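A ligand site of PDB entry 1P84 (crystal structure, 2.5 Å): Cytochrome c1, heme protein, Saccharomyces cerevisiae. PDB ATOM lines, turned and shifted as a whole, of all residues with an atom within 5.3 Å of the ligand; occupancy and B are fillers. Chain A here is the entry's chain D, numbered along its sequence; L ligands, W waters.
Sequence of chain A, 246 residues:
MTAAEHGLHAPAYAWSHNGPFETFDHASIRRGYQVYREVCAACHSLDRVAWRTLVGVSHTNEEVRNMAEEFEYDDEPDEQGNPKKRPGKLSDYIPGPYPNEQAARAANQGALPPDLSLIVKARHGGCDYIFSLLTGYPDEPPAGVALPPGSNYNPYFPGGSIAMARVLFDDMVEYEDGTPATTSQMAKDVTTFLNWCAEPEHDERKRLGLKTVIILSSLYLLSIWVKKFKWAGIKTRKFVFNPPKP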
ATOM      1  N   VAL A  35     -41.375  -9.298 -30.613  1.00  0.00           N
ATOM      2  CA  VAL A  35     -40.070  -9.677 -31.127  1.00  0.00           C
ATOM      3  C   VAL A  35     -39.255 -10.282 -30.004  1.00  0.00           C
ATOM      4  O   VAL A  35     -38.474 -11.211 -30.219  1.00  0.00           O
ATOM      5  CB  VAL A  35     -39.317  -8.482 -31.703  1.00  0.00           C
ATOM      6  CG1 VAL A  35     -37.953  -8.912 -32.212  1.00  0.00           C
ATOM      7  CG2 VAL A  35     -40.115  -7.849 -32.823  1.00  0.00           C
ATOM      8  N   VAL A  39     -38.323 -14.163 -30.479  1.00  0.00           N
ATOM      9  CA  VAL A  39     -36.925 -14.333 -30.860  1.00  0.00           C
ATOM     10  C   VAL A  39     -35.940 -14.372 -29.683  1.00  0.00           C
ATOM     11  O   VAL A  39     -35.340 -15.419 -29.398  1.00  0.00           O
ATOM     12  CB  VAL A  39     -36.471 -13.216 -31.840  1.00  0.00           C
ATOM     13  CG1 VAL A  39     -35.055 -13.478 -32.325  1.00  0.00           C
ATOM     14  CG2 VAL A  39     -37.422 -13.125 -33.025  1.00  0.00           C
ATOM     15  N   CYS A  40     -35.826 -13.244 -28.984  1.00  0.00           N
ATOM     16  CA  CYS A  40     -34.894 -13.077 -27.886  1.00  0.00           C
ATOM     17  C   CYS A  40     -35.074 -13.925 -26.630  1.00  0.00           C
ATOM     18  O   CYS A  40     -34.087 -14.447 -26.100  1.00  0.00           O
ATOM     19  CB  CYS A  40     -34.839 -11.598 -27.500  1.00  0.00           C
ATOM     20  SG  CYS A  40     -34.951 -10.469 -28.916  1.00  0.00           S
ATOM     21  N   ALA A  42     -35.639 -16.750 -26.119  1.00  0.00           N
ATOM     22  CA  ALA A  42     -35.069 -18.079 -26.234  1.00  0.00           C
ATOM     23  C   ALA A  42     -33.741 -18.176 -25.485  1.00  0.00           C
ATOM     24  O   ALA A  42     -33.383 -19.250 -24.984  1.00  0.00           O
ATOM     25  CB  ALA A  42     -34.860 -18.413 -27.705  1.00  0.00           C
ATOM     26  N   CYS A  43     -33.032 -17.050 -25.394  1.00  0.00           N
ATOM     27  CA  CYS A  43     -31.742 -17.007 -24.708  1.00  0.00           C
ATOM     28  C   CYS A  43     -31.584 -15.879 -23.665  1.00  0.00           C
ATOM     29  O   CYS A  43     -30.702 -15.950 -22.807  1.00  0.00           O
ATOM     30  CB  CYS A  43     -30.601 -16.867 -25.725  1.00  0.00           C
ATOM     31  SG  CYS A  43     -30.822 -17.822 -27.258  1.00  0.00           S
ATOM     32  N   HIS A  44     -32.436 -14.854 -23.744  1.00  0.00           N
ATOM     33  CA  HIS A  44     -32.361 -13.725 -22.830  1.00  0.00           C
ATOM     34  C   HIS A  44     -33.490 -13.606 -21.819  1.00  0.00           C
ATOM     35  O   HIS A  44     -34.664 -13.644 -22.163  1.00  0.00           O
ATOM     36  CB  HIS A  44     -32.309 -12.405 -23.620  1.00  0.00           C
ATOM     37  CG  HIS A  44     -31.006 -12.156 -24.321  1.00  0.00           C
ATOM     38  ND1 HIS A  44     -29.807 -11.982 -23.675  1.00  0.00           N
ATOM     39  CD2 HIS A  44     -30.743 -12.022 -25.638  1.00  0.00           C
ATOM     40  CE1 HIS A  44     -28.870 -11.751 -24.608  1.00  0.00           C
ATOM     41  NE2 HIS A  44     -29.387 -11.776 -25.821  1.00  0.00           N
ATOM     42  N   ASN A 108     -24.976 -22.131 -24.804  1.00  0.00           N
ATOM     43  CA  ASN A 108     -24.412 -21.072 -25.644  1.00  0.00           C
ATOM     44  C   ASN A 108     -22.894 -21.091 -25.828  1.00  0.00           C
ATOM     45  O   ASN A 108     -22.256 -20.040 -25.832  1.00  0.00           O
ATOM     46  CB  ASN A 108     -24.844 -19.689 -25.131  1.00  0.00           C
ATOM     47  CG  ASN A 108     -26.321 -19.454 -25.266  1.00  0.00           C
ATOM     48  OD1 ASN A 108     -26.811 -19.079 -26.335  1.00  0.00           O
ATOM     49  ND2 ASN A 108     -27.065 -19.698 -24.188  1.00  0.00           N
ATOM     50  N   ALA A 111     -20.971 -19.129 -23.302  1.00  0.00           N
ATOM     51  CA  ALA A 111     -21.219 -17.707 -23.147  1.00  0.00           C
ATOM     52  C   ALA A 111     -22.481 -17.494 -22.317  1.00  0.00           C
ATOM     53  O   ALA A 111     -23.343 -18.372 -22.227  1.00  0.00           O
ATOM     54  CB  ALA A 111     -21.362 -17.042 -24.493  1.00  0.00           C
ATOM     55  N   LEU A 112     -22.602 -16.318 -21.720  1.00  0.00           N
ATOM     56  CA  LEU A 112     -23.757 -16.007 -20.891  1.00  0.00           C
ATOM     57  C   LEU A 112     -24.566 -14.844 -21.442  1.00  0.00           C
ATOM     58  O   LEU A 112     -24.133 -13.703 -21.384  1.00  0.00           O
ATOM     59  CB  LEU A 112     -23.257 -15.674 -19.480  1.00  0.00           C
ATOM     60  CG  LEU A 112     -24.262 -15.387 -18.362  1.00  0.00           C
ATOM     61  CD1 LEU A 112     -25.171 -16.583 -18.120  1.00  0.00           C
ATOM     62  CD2 LEU A 112     -23.478 -15.029 -17.109  1.00  0.00           C
ATOM     63  N   PRO A 113     -25.742 -15.135 -22.017  1.00  0.00           N
ATOM     64  CA  PRO A 113     -26.573 -14.059 -22.564  1.00  0.00           C
ATOM     65  C   PRO A 113     -27.009 -13.216 -21.365  1.00  0.00           C
ATOM     66  O   PRO A 113     -27.665 -13.729 -20.461  1.00  0.00           O
ATOM     67  CB  PRO A 113     -27.758 -14.810 -23.164  1.00  0.00           C
ATOM     68  CG  PRO A 113     -27.221 -16.188 -23.423  1.00  0.00           C
ATOM     69  CD  PRO A 113     -26.373 -16.446 -22.212  1.00  0.00           C
ATOM     70  N   PRO A 114     -26.614 -11.937 -21.317  1.00  0.00           N
ATOM     71  CA  PRO A 114     -27.000 -11.100 -20.182  1.00  0.00           C
ATOM     72  C   PRO A 114     -28.487 -10.780 -20.128  1.00  0.00           C
ATOM     73  O   PRO A 114     -29.205 -10.917 -21.114  1.00  0.00           O
ATOM     74  CB  PRO A 114     -26.178  -9.836 -20.404  1.00  0.00           C
ATOM     75  CG  PRO A 114     -26.122  -9.746 -21.881  1.00  0.00           C
ATOM     76  CD  PRO A 114     -25.791 -11.163 -22.266  1.00  0.00           C
ATOM     77  N   LEU A 116     -31.636  -8.501 -20.180  1.00  0.00           N
ATOM     78  CA  LEU A 116     -31.883  -7.268 -20.939  1.00  0.00           C
ATOM     79  C   LEU A 116     -32.690  -6.159 -20.243  1.00  0.00           C
ATOM     80  O   LEU A 116     -32.941  -5.111 -20.842  1.00  0.00           O
ATOM     81  CB  LEU A 116     -32.538  -7.602 -22.289  1.00  0.00           C
ATOM     82  CG  LEU A 116     -31.768  -8.516 -23.243  1.00  0.00           C
ATOM     83  CD1 LEU A 116     -32.540  -8.658 -24.555  1.00  0.00           C
ATOM     84  CD2 LEU A 116     -30.376  -7.956 -23.516  1.00  0.00           C
ATOM     85  N   ILE A 119     -30.090  -3.324 -20.029  1.00  0.00           N
ATOM     86  CA  ILE A 119     -29.141  -3.251 -21.138  1.00  0.00           C
ATOM     87  C   ILE A 119     -28.985  -1.883 -21.820  1.00  0.00           C
ATOM     88  O   ILE A 119     -27.872  -1.492 -22.140  1.00  0.00           O
ATOM     89  CB  ILE A 119     -29.401  -4.374 -22.189  1.00  0.00           C
ATOM     90  CG1 ILE A 119     -28.063  -4.912 -22.693  1.00  0.00           C
ATOM     91  CG2 ILE A 119     -30.252  -3.873 -23.361  1.00  0.00           C
ATOM     92  CD1 ILE A 119     -27.225  -5.552 -21.605  1.00  0.00           C
ATOM     93  N   ARG A 123     -24.874   0.392 -21.247  1.00  0.00           N
ATOM     94  CA  ARG A 123     -23.931   0.438 -22.369  1.00  0.00           C
ATOM     95  C   ARG A 123     -23.867   1.848 -22.943  1.00  0.00           C
ATOM     96  O   ARG A 123     -24.916   2.487 -23.133  1.00  0.00           O
ATOM     97  CB  ARG A 123     -24.363  -0.503 -23.501  1.00  0.00           C
ATOM     98  CG  ARG A 123     -24.476  -1.981 -23.169  1.00  0.00           C
ATOM     99  CD  ARG A 123     -23.119  -2.627 -22.984  1.00  0.00           C
ATOM    100  NE  ARG A 123     -23.209  -4.089 -22.895  1.00  0.00           N
ATOM    101  CZ  ARG A 123     -23.462  -4.765 -21.779  1.00  0.00           C
ATOM    102  NH1 ARG A 123     -23.528  -6.087 -21.813  1.00  0.00           N
ATOM    103  NH2 ARG A 123     -23.641  -4.135 -20.626  1.00  0.00           N
ATOM    104  N   TYR A 129     -26.638   2.067 -29.907  1.00  0.00           N
ATOM    105  CA  TYR A 129     -25.755   0.923 -29.855  1.00  0.00           C
ATOM    106  C   TYR A 129     -26.483  -0.407 -30.080  1.00  0.00           C
ATOM    107  O   TYR A 129     -26.072  -1.195 -30.917  1.00  0.00           O
ATOM    108  CB  TYR A 129     -24.998   0.877 -28.517  1.00  0.00           C
ATOM    109  CG  TYR A 129     -24.229  -0.403 -28.306  1.00  0.00           C
ATOM    110  CD1 TYR A 129     -23.112  -0.702 -29.089  1.00  0.00           C
ATOM    111  CD2 TYR A 129     -24.650  -1.346 -27.378  1.00  0.00           C
ATOM    112  CE1 TYR A 129     -22.454  -1.931 -28.954  1.00  0.00           C
ATOM    113  CE2 TYR A 129     -24.002  -2.572 -27.243  1.00  0.00           C
ATOM    114  CZ  TYR A 129     -22.910  -2.847 -28.041  1.00  0.00           C
ATOM    115  OH  TYR A 129     -22.279  -4.055 -27.910  1.00  0.00           O
ATOM    116  N   ILE A 130     -27.548  -0.652 -29.319  1.00  0.00           N
ATOM    117  CA  ILE A 130     -28.317  -1.902 -29.426  1.00  0.00           C
ATOM    118  C   ILE A 130     -28.807  -2.151 -30.854  1.00  0.00           C
ATOM    119  O   ILE A 130     -28.656  -3.245 -31.402  1.00  0.00           O
ATOM    120  CB  ILE A 130     -29.543  -1.923 -28.475  1.00  0.00           C
ATOM    121  CG1 ILE A 130     -29.111  -1.701 -27.032  1.00  0.00           C
ATOM    122  CG2 ILE A 130     -30.271  -3.257 -28.592  1.00  0.00           C
ATOM    123  CD1 ILE A 130     -28.174  -2.763 -26.500  1.00  0.00           C
ATOM    124  N   LEU A 133     -25.873  -2.816 -33.266  1.00  0.00           N
ATOM    125  CA  LEU A 133     -25.291  -4.143 -33.072  1.00  0.00           C
ATOM    126  C   LEU A 133     -26.140  -5.202 -33.771  1.00  0.00           C
ATOM    127  O   LEU A 133     -25.625  -6.070 -34.491  1.00  0.00           O
ATOM    128  CB  LEU A 133     -25.187  -4.464 -31.569  1.00  0.00           C
ATOM    129  CG  LEU A 133     -24.569  -5.816 -31.218  1.00  0.00           C
ATOM    130  CD1 LEU A 133     -23.058  -5.702 -31.125  1.00  0.00           C
ATOM    131  CD2 LEU A 133     -25.127  -6.316 -29.904  1.00  0.00           C
ATOM    132  N   LEU A 134     -27.459  -5.124 -33.576  1.00  0.00           N
ATOM    133  CA  LEU A 134     -28.403  -6.071 -34.149  1.00  0.00           C
ATOM    134  C   LEU A 134     -28.457  -6.090 -35.673  1.00  0.00           C
ATOM    135  O   LEU A 134     -28.587  -7.155 -36.281  1.00  0.00           O
ATOM    136  CB  LEU A 134     -29.815  -5.834 -33.586  1.00  0.00           C
ATOM    137  CG  LEU A 134     -30.076  -6.216 -32.125  1.00  0.00           C
ATOM    138  CD1 LEU A 134     -31.465  -5.757 -31.716  1.00  0.00           C
ATOM    139  CD2 LEU A 134     -29.934  -7.703 -31.936  1.00  0.00           C
ATOM    140  N   PHE A 157     -19.335  -4.147 -31.747  1.00  0.00           N
ATOM    141  CA  PHE A 157     -18.959  -4.785 -30.486  1.00  0.00           C
ATOM    142  C   PHE A 157     -17.440  -4.637 -30.301  1.00  0.00           C
ATOM    143  O   PHE A 157     -16.683  -4.805 -31.250  1.00  0.00           O
ATOM    144  CB  PHE A 157     -19.369  -6.249 -30.518  1.00  0.00           C
ATOM    145  CG  PHE A 157     -19.170  -6.976 -29.215  1.00  0.00           C
ATOM    146  CD1 PHE A 157     -20.085  -6.824 -28.169  1.00  0.00           C
ATOM    147  CD2 PHE A 157     -18.091  -7.830 -29.039  1.00  0.00           C
ATOM    148  CE1 PHE A 157     -19.919  -7.516 -26.974  1.00  0.00           C
ATOM    149  CE2 PHE A 157     -17.918  -8.537 -27.839  1.00  0.00           C
ATOM    150  CZ  PHE A 157     -18.830  -8.369 -26.808  1.00  0.00           C
ATOM    151  N   SER A 161     -15.182  -9.640 -31.940  1.00  0.00           N
ATOM    152  CA  SER A 161     -15.630 -11.011 -31.760  1.00  0.00           C
ATOM    153  C   SER A 161     -16.739 -11.190 -30.702  1.00  0.00           C
ATOM    154  O   SER A 161     -16.484 -11.142 -29.494  1.00  0.00           O
ATOM    155  CB  SER A 161     -14.445 -11.898 -31.423  1.00  0.00           C
ATOM    156  OG  SER A 161     -14.871 -13.225 -31.178  1.00  0.00           O
ATOM    157  N   ILE A 162     -17.963 -11.428 -31.170  1.00  0.00           N
ATOM    158  CA  ILE A 162     -19.125 -11.611 -30.294  1.00  0.00           C
ATOM    159  C   ILE A 162     -19.663 -13.050 -30.361  1.00  0.00           C
ATOM    160  O   ILE A 162     -19.624 -13.669 -31.414  1.00  0.00           O
ATOM    161  CB  ILE A 162     -20.239 -10.599 -30.646  1.00  0.00           C
ATOM    162  CG1 ILE A 162     -21.352 -10.630 -29.590  1.00  0.00           C
ATOM    163  CG2 ILE A 162     -20.788 -10.883 -32.041  1.00  0.00           C
ATOM    164  CD1 ILE A 162     -22.353  -9.497 -29.724  1.00  0.00           C
ATOM    165  N   ALA A 163     -20.151 -13.552 -29.227  1.00  0.00           N
ATOM    166  CA  ALA A 163     -20.678 -14.911 -29.126  1.00  0.00           C
ATOM    167  C   ALA A 163     -22.148 -15.059 -29.537  1.00  0.00           C
ATOM    168  O   ALA A 163     -22.730 -16.137 -29.407  1.00  0.00           O
ATOM    169  CB  ALA A 163     -20.456 -15.460 -27.733  1.00  0.00           C
ATOM    170  N   MET A 164     -22.749 -13.975 -30.002  1.00  0.00           N
ATOM    171  CA  MET A 164     -24.137 -14.001 -30.428  1.00  0.00           C
ATOM    172  C   MET A 164     -24.144 -13.869 -31.937  1.00  0.00           C
ATOM    173  O   MET A 164     -23.497 -12.983 -32.494  1.00  0.00           O
ATOM    174  CB  MET A 164     -24.944 -12.849 -29.801  1.00  0.00           C
ATOM    175  CG  MET A 164     -26.394 -12.747 -30.298  1.00  0.00           C
ATOM    176  SD  MET A 164     -27.445 -11.552 -29.414  1.00  0.00           S
ATOM    177  CE  MET A 164     -27.490 -10.153 -30.519  1.00  0.00           C
ATOM    178  N   VAL A 167     -29.586 -12.940 -35.403  1.00  0.00           N
ATOM    179  CA  VAL A 167     -30.825 -13.677 -35.148  1.00  0.00           C
ATOM    180  C   VAL A 167     -32.038 -13.065 -35.826  1.00  0.00           C
ATOM    181  O   VAL A 167     -33.105 -13.682 -35.874  1.00  0.00           O
ATOM    182  CB  VAL A 167     -31.130 -13.861 -33.649  1.00  0.00           C
ATOM    183  CG1 VAL A 167     -29.982 -14.567 -32.952  1.00  0.00           C
ATOM    184  CG2 VAL A 167     -31.428 -12.524 -32.989  1.00  0.00           C
ATOM    185  N   LEU A 168     -31.898 -11.851 -36.335  1.00  0.00           N
ATOM    186  CA  LEU A 168     -33.008 -11.200 -37.008  1.00  0.00           C
ATOM    187  C   LEU A 168     -32.828 -11.317 -38.519  1.00  0.00           C
ATOM    188  O   LEU A 168     -31.762 -10.989 -39.068  1.00  0.00           O
ATOM    189  CB  LEU A 168     -33.116  -9.713 -36.603  1.00  0.00           C
ATOM    190  CG  LEU A 168     -33.345  -9.373 -35.132  1.00  0.00           C
ATOM    191  CD1 LEU A 168     -33.584  -7.871 -34.985  1.00  0.00           C
ATOM    192  CD2 LEU A 168     -34.531 -10.151 -34.593  1.00  0.00           C
ATOM    193  N   VAL A 190     -37.713  -3.835 -30.846  1.00  0.00           N
ATOM    194  CA  VAL A 190     -37.210  -4.413 -29.590  1.00  0.00           C
ATOM    195  C   VAL A 190     -36.438  -3.380 -28.767  1.00  0.00           C
ATOM    196  O   VAL A 190     -36.629  -3.260 -27.551  1.00  0.00           O
ATOM    197  CB  VAL A 190     -36.225  -5.603 -29.788  1.00  0.00           C
ATOM    198  CG1 VAL A 190     -36.902  -6.903 -29.589  1.00  0.00           C
ATOM    199  CG2 VAL A 190     -35.554  -5.523 -31.131  1.00  0.00           C
ATOM    200  N   LEU A 194     -36.965  -2.326 -25.132  1.00  0.00           N
ATOM    201  CA  LEU A 194     -35.896  -2.520 -24.155  1.00  0.00           C
ATOM    202  C   LEU A 194     -35.570  -1.204 -23.440  1.00  0.00           C
ATOM    203  O   LEU A 194     -35.144  -1.209 -22.283  1.00  0.00           O
ATOM    204  CB  LEU A 194     -34.667  -3.122 -24.807  1.00  0.00           C
ATOM    205  CG  LEU A 194     -34.842  -4.586 -25.209  1.00  0.00           C
ATOM    206  CD1 LEU A 194     -33.523  -5.162 -25.720  1.00  0.00           C
ATOM    207  CD2 LEU A 194     -35.359  -5.378 -24.018  1.00  0.00           C
HETATM  208 FE1  LIG L   1     -28.445 -11.721 -27.552  1.00  0.00          FE
HETATM  209  C1  LIG L   1     -25.576 -10.756 -25.966  1.00  0.00           C
HETATM  210  C2  LIG L   1     -29.489  -8.453 -27.574  1.00  0.00           C
HETATM  211  C3  LIG L   1     -31.261 -12.592 -29.322  1.00  0.00           C
HETATM  212  C4  LIG L   1     -27.530 -14.972 -27.350  1.00  0.00           C
HETATM  213  N1  LIG L   1     -27.678  -9.945 -26.944  1.00  0.00           N
HETATM  214  C5  LIG L   1     -26.485  -9.751 -26.289  1.00  0.00           C
HETATM  215  C6  LIG L   1     -26.338  -8.361 -25.933  1.00  0.00           C
HETATM  216  C7  LIG L   1     -27.385  -7.704 -26.455  1.00  0.00           C
HETATM  217  C8  LIG L   1     -28.261  -8.705 -27.022  1.00  0.00           C
HETATM  218  C9  LIG L   1     -27.618  -6.218 -26.423  1.00  0.00           C
HETATM  219  C10 LIG L   1     -25.245  -7.739 -25.125  1.00  0.00           C
HETATM  220  C11 LIG L   1     -24.100  -7.373 -26.021  1.00  0.00           C
HETATM  221  C12 LIG L   1     -23.107  -6.483 -25.326  1.00  0.00           C
HETATM  222  O1  LIG L   1     -22.474  -6.948 -24.358  1.00  0.00           O
HETATM  223  O2  LIG L   1     -22.968  -5.319 -25.748  1.00  0.00           O
HETATM  224  N2  LIG L   1     -30.049 -10.730 -28.281  1.00  0.00           N
HETATM  225  C13 LIG L   1     -30.340  -9.395 -28.135  1.00  0.00           C
HETATM  226  C14 LIG L   1     -31.685  -9.118 -28.578  1.00  0.00           C
HETATM  227  C15 LIG L   1     -32.138 -10.245 -29.147  1.00  0.00           C
HETATM  228  C16 LIG L   1     -31.118 -11.257 -28.990  1.00  0.00           C
HETATM  229  C17 LIG L   1     -32.436  -7.814 -28.460  1.00  0.00           C
HETATM  230  C18 LIG L   1     -33.442 -10.553 -29.862  1.00  0.00           C
HETATM  231  C19 LIG L   1     -33.615  -9.597 -31.040  1.00  0.00           C
HETATM  232  N3  LIG L   1     -29.240 -13.441 -28.216  1.00  0.00           N
HETATM  233  C20 LIG L   1     -30.386 -13.609 -28.953  1.00  0.00           C
HETATM  234  C21 LIG L   1     -30.672 -15.029 -29.073  1.00  0.00           C
HETATM  235  C22 LIG L   1     -29.669 -15.693 -28.461  1.00  0.00           C
HETATM  236  C23 LIG L   1     -28.733 -14.698 -27.988  1.00  0.00           C
HETATM  237  C24 LIG L   1     -31.921 -15.659 -29.681  1.00  0.00           C
HETATM  238  C25 LIG L   1     -29.428 -17.158 -28.175  1.00  0.00           C
HETATM  239  C26 LIG L   1     -29.297 -18.026 -29.426  1.00  0.00           C
HETATM  240  N4  LIG L   1     -26.871 -12.666 -26.807  1.00  0.00           N
HETATM  241  C27 LIG L   1     -26.657 -14.023 -26.816  1.00  0.00           C
HETATM  242  C28 LIG L   1     -25.325 -14.312 -26.314  1.00  0.00           C
HETATM  243  C29 LIG L   1     -24.765 -13.124 -25.960  1.00  0.00           C
HETATM  244  C30 LIG L   1     -25.753 -12.106 -26.220  1.00  0.00           C
HETATM  245  C31 LIG L   1     -24.720 -15.710 -26.248  1.00  0.00           C
HETATM  246  C32 LIG L   1     -23.356 -12.886 -25.419  1.00  0.00           C
HETATM  247  C33 LIG L   1     -22.416 -12.098 -26.339  1.00  0.00           C
HETATM  248  C34 LIG L   1     -20.997 -11.949 -25.780  1.00  0.00           C
HETATM  249  O3  LIG L   1     -20.829 -11.792 -24.544  1.00  0.00           O
HETATM  250  O4  LIG L   1     -20.043 -11.988 -26.576  1.00  0.00           O
HETATM  251  O   HOH W   1     -22.703  -9.577 -23.816  1.00  0.00           O
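Val 39 touches the ligand.
Asn 108 touches the ligand.
Pro 113 touches the ligand.
Pro 114 touches the ligand (CD to C1, 3.7 Å).
CD1 of Leu 116 touches C17 of the ligand, at 3.997 Å.
Ile 119 touches the ligand (CG1 to C9, 3.98 Å).
Ile 130 touches the ligand (CD1 to C9, 3.5 Å).
Leu 134 touches the ligand.
CE1 of Phe 157 touches O1 of the ligand (3.7 Å).
Ile 162 touches the ligand (CG1 to O4, 3.6 Å).
Val 167 touches the ligand.
Leu 168 touches the ligand.
Leu 194 touches the ligand.
Hydrophobic or aromatic side chains that line the ligand: His 44, Pro 113, Pro 114, Leu 116, Ile 119, Tyr 129, Ile 130, Leu 134, Phe 157, Ile 162, Ala 163, Met 164, Val 167, Leu 168 and Leu 194.
Within 4 Å of the ligand: Val 39, Cys 40, Cys 43, His 44, Asn 108, Pro 113, Pro 114, Leu 116, Ile 119, Arg 123, Tyr 129, Ile 130, Leu 134, Phe 157, Ile 162, Ala 163, Met 164, Val 167, Leu 168 and Leu 194.
Along chain A the residues within 4 Å of the ligand span positions 39 to 194.
The side-chain sulfur of Cys 40 is bonded to a carbon (C18) of the ligand (1.8 Å).
A carbon (C25) of the ligand is bonded to the side-chain sulfur (SG) of Cys 43, 1.8 Å away.
A ring nitrogen (NE2) of His 44 is bound to an iron atom (FE1) of the ligand (2.0 Å).
An iron atom (FE1) of the ligand is bound by the side-chain sulfur of Met 164 (2.1 Å).
The side-chain hydroxyl of Tyr 129 sits at hydrogen-bond distance from an oxygen (O2) of the ligand, at 2.6 Å.
An oxygen (O1) of the ligand is in salt-bridge range of the guanidinium group (NH1) of Arg 123, at 2.9 Å.
An oxygen (O4) of the ligand sits at hydrogen-bond distance from the backbone NH of Ala 163 (3.1 Å).
A ring nitrogen (ND1) of His 44 lies within hydrogen-bond range of the backbone carbonyl oxygen (O) of Pro 114, at 2.8 Å.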
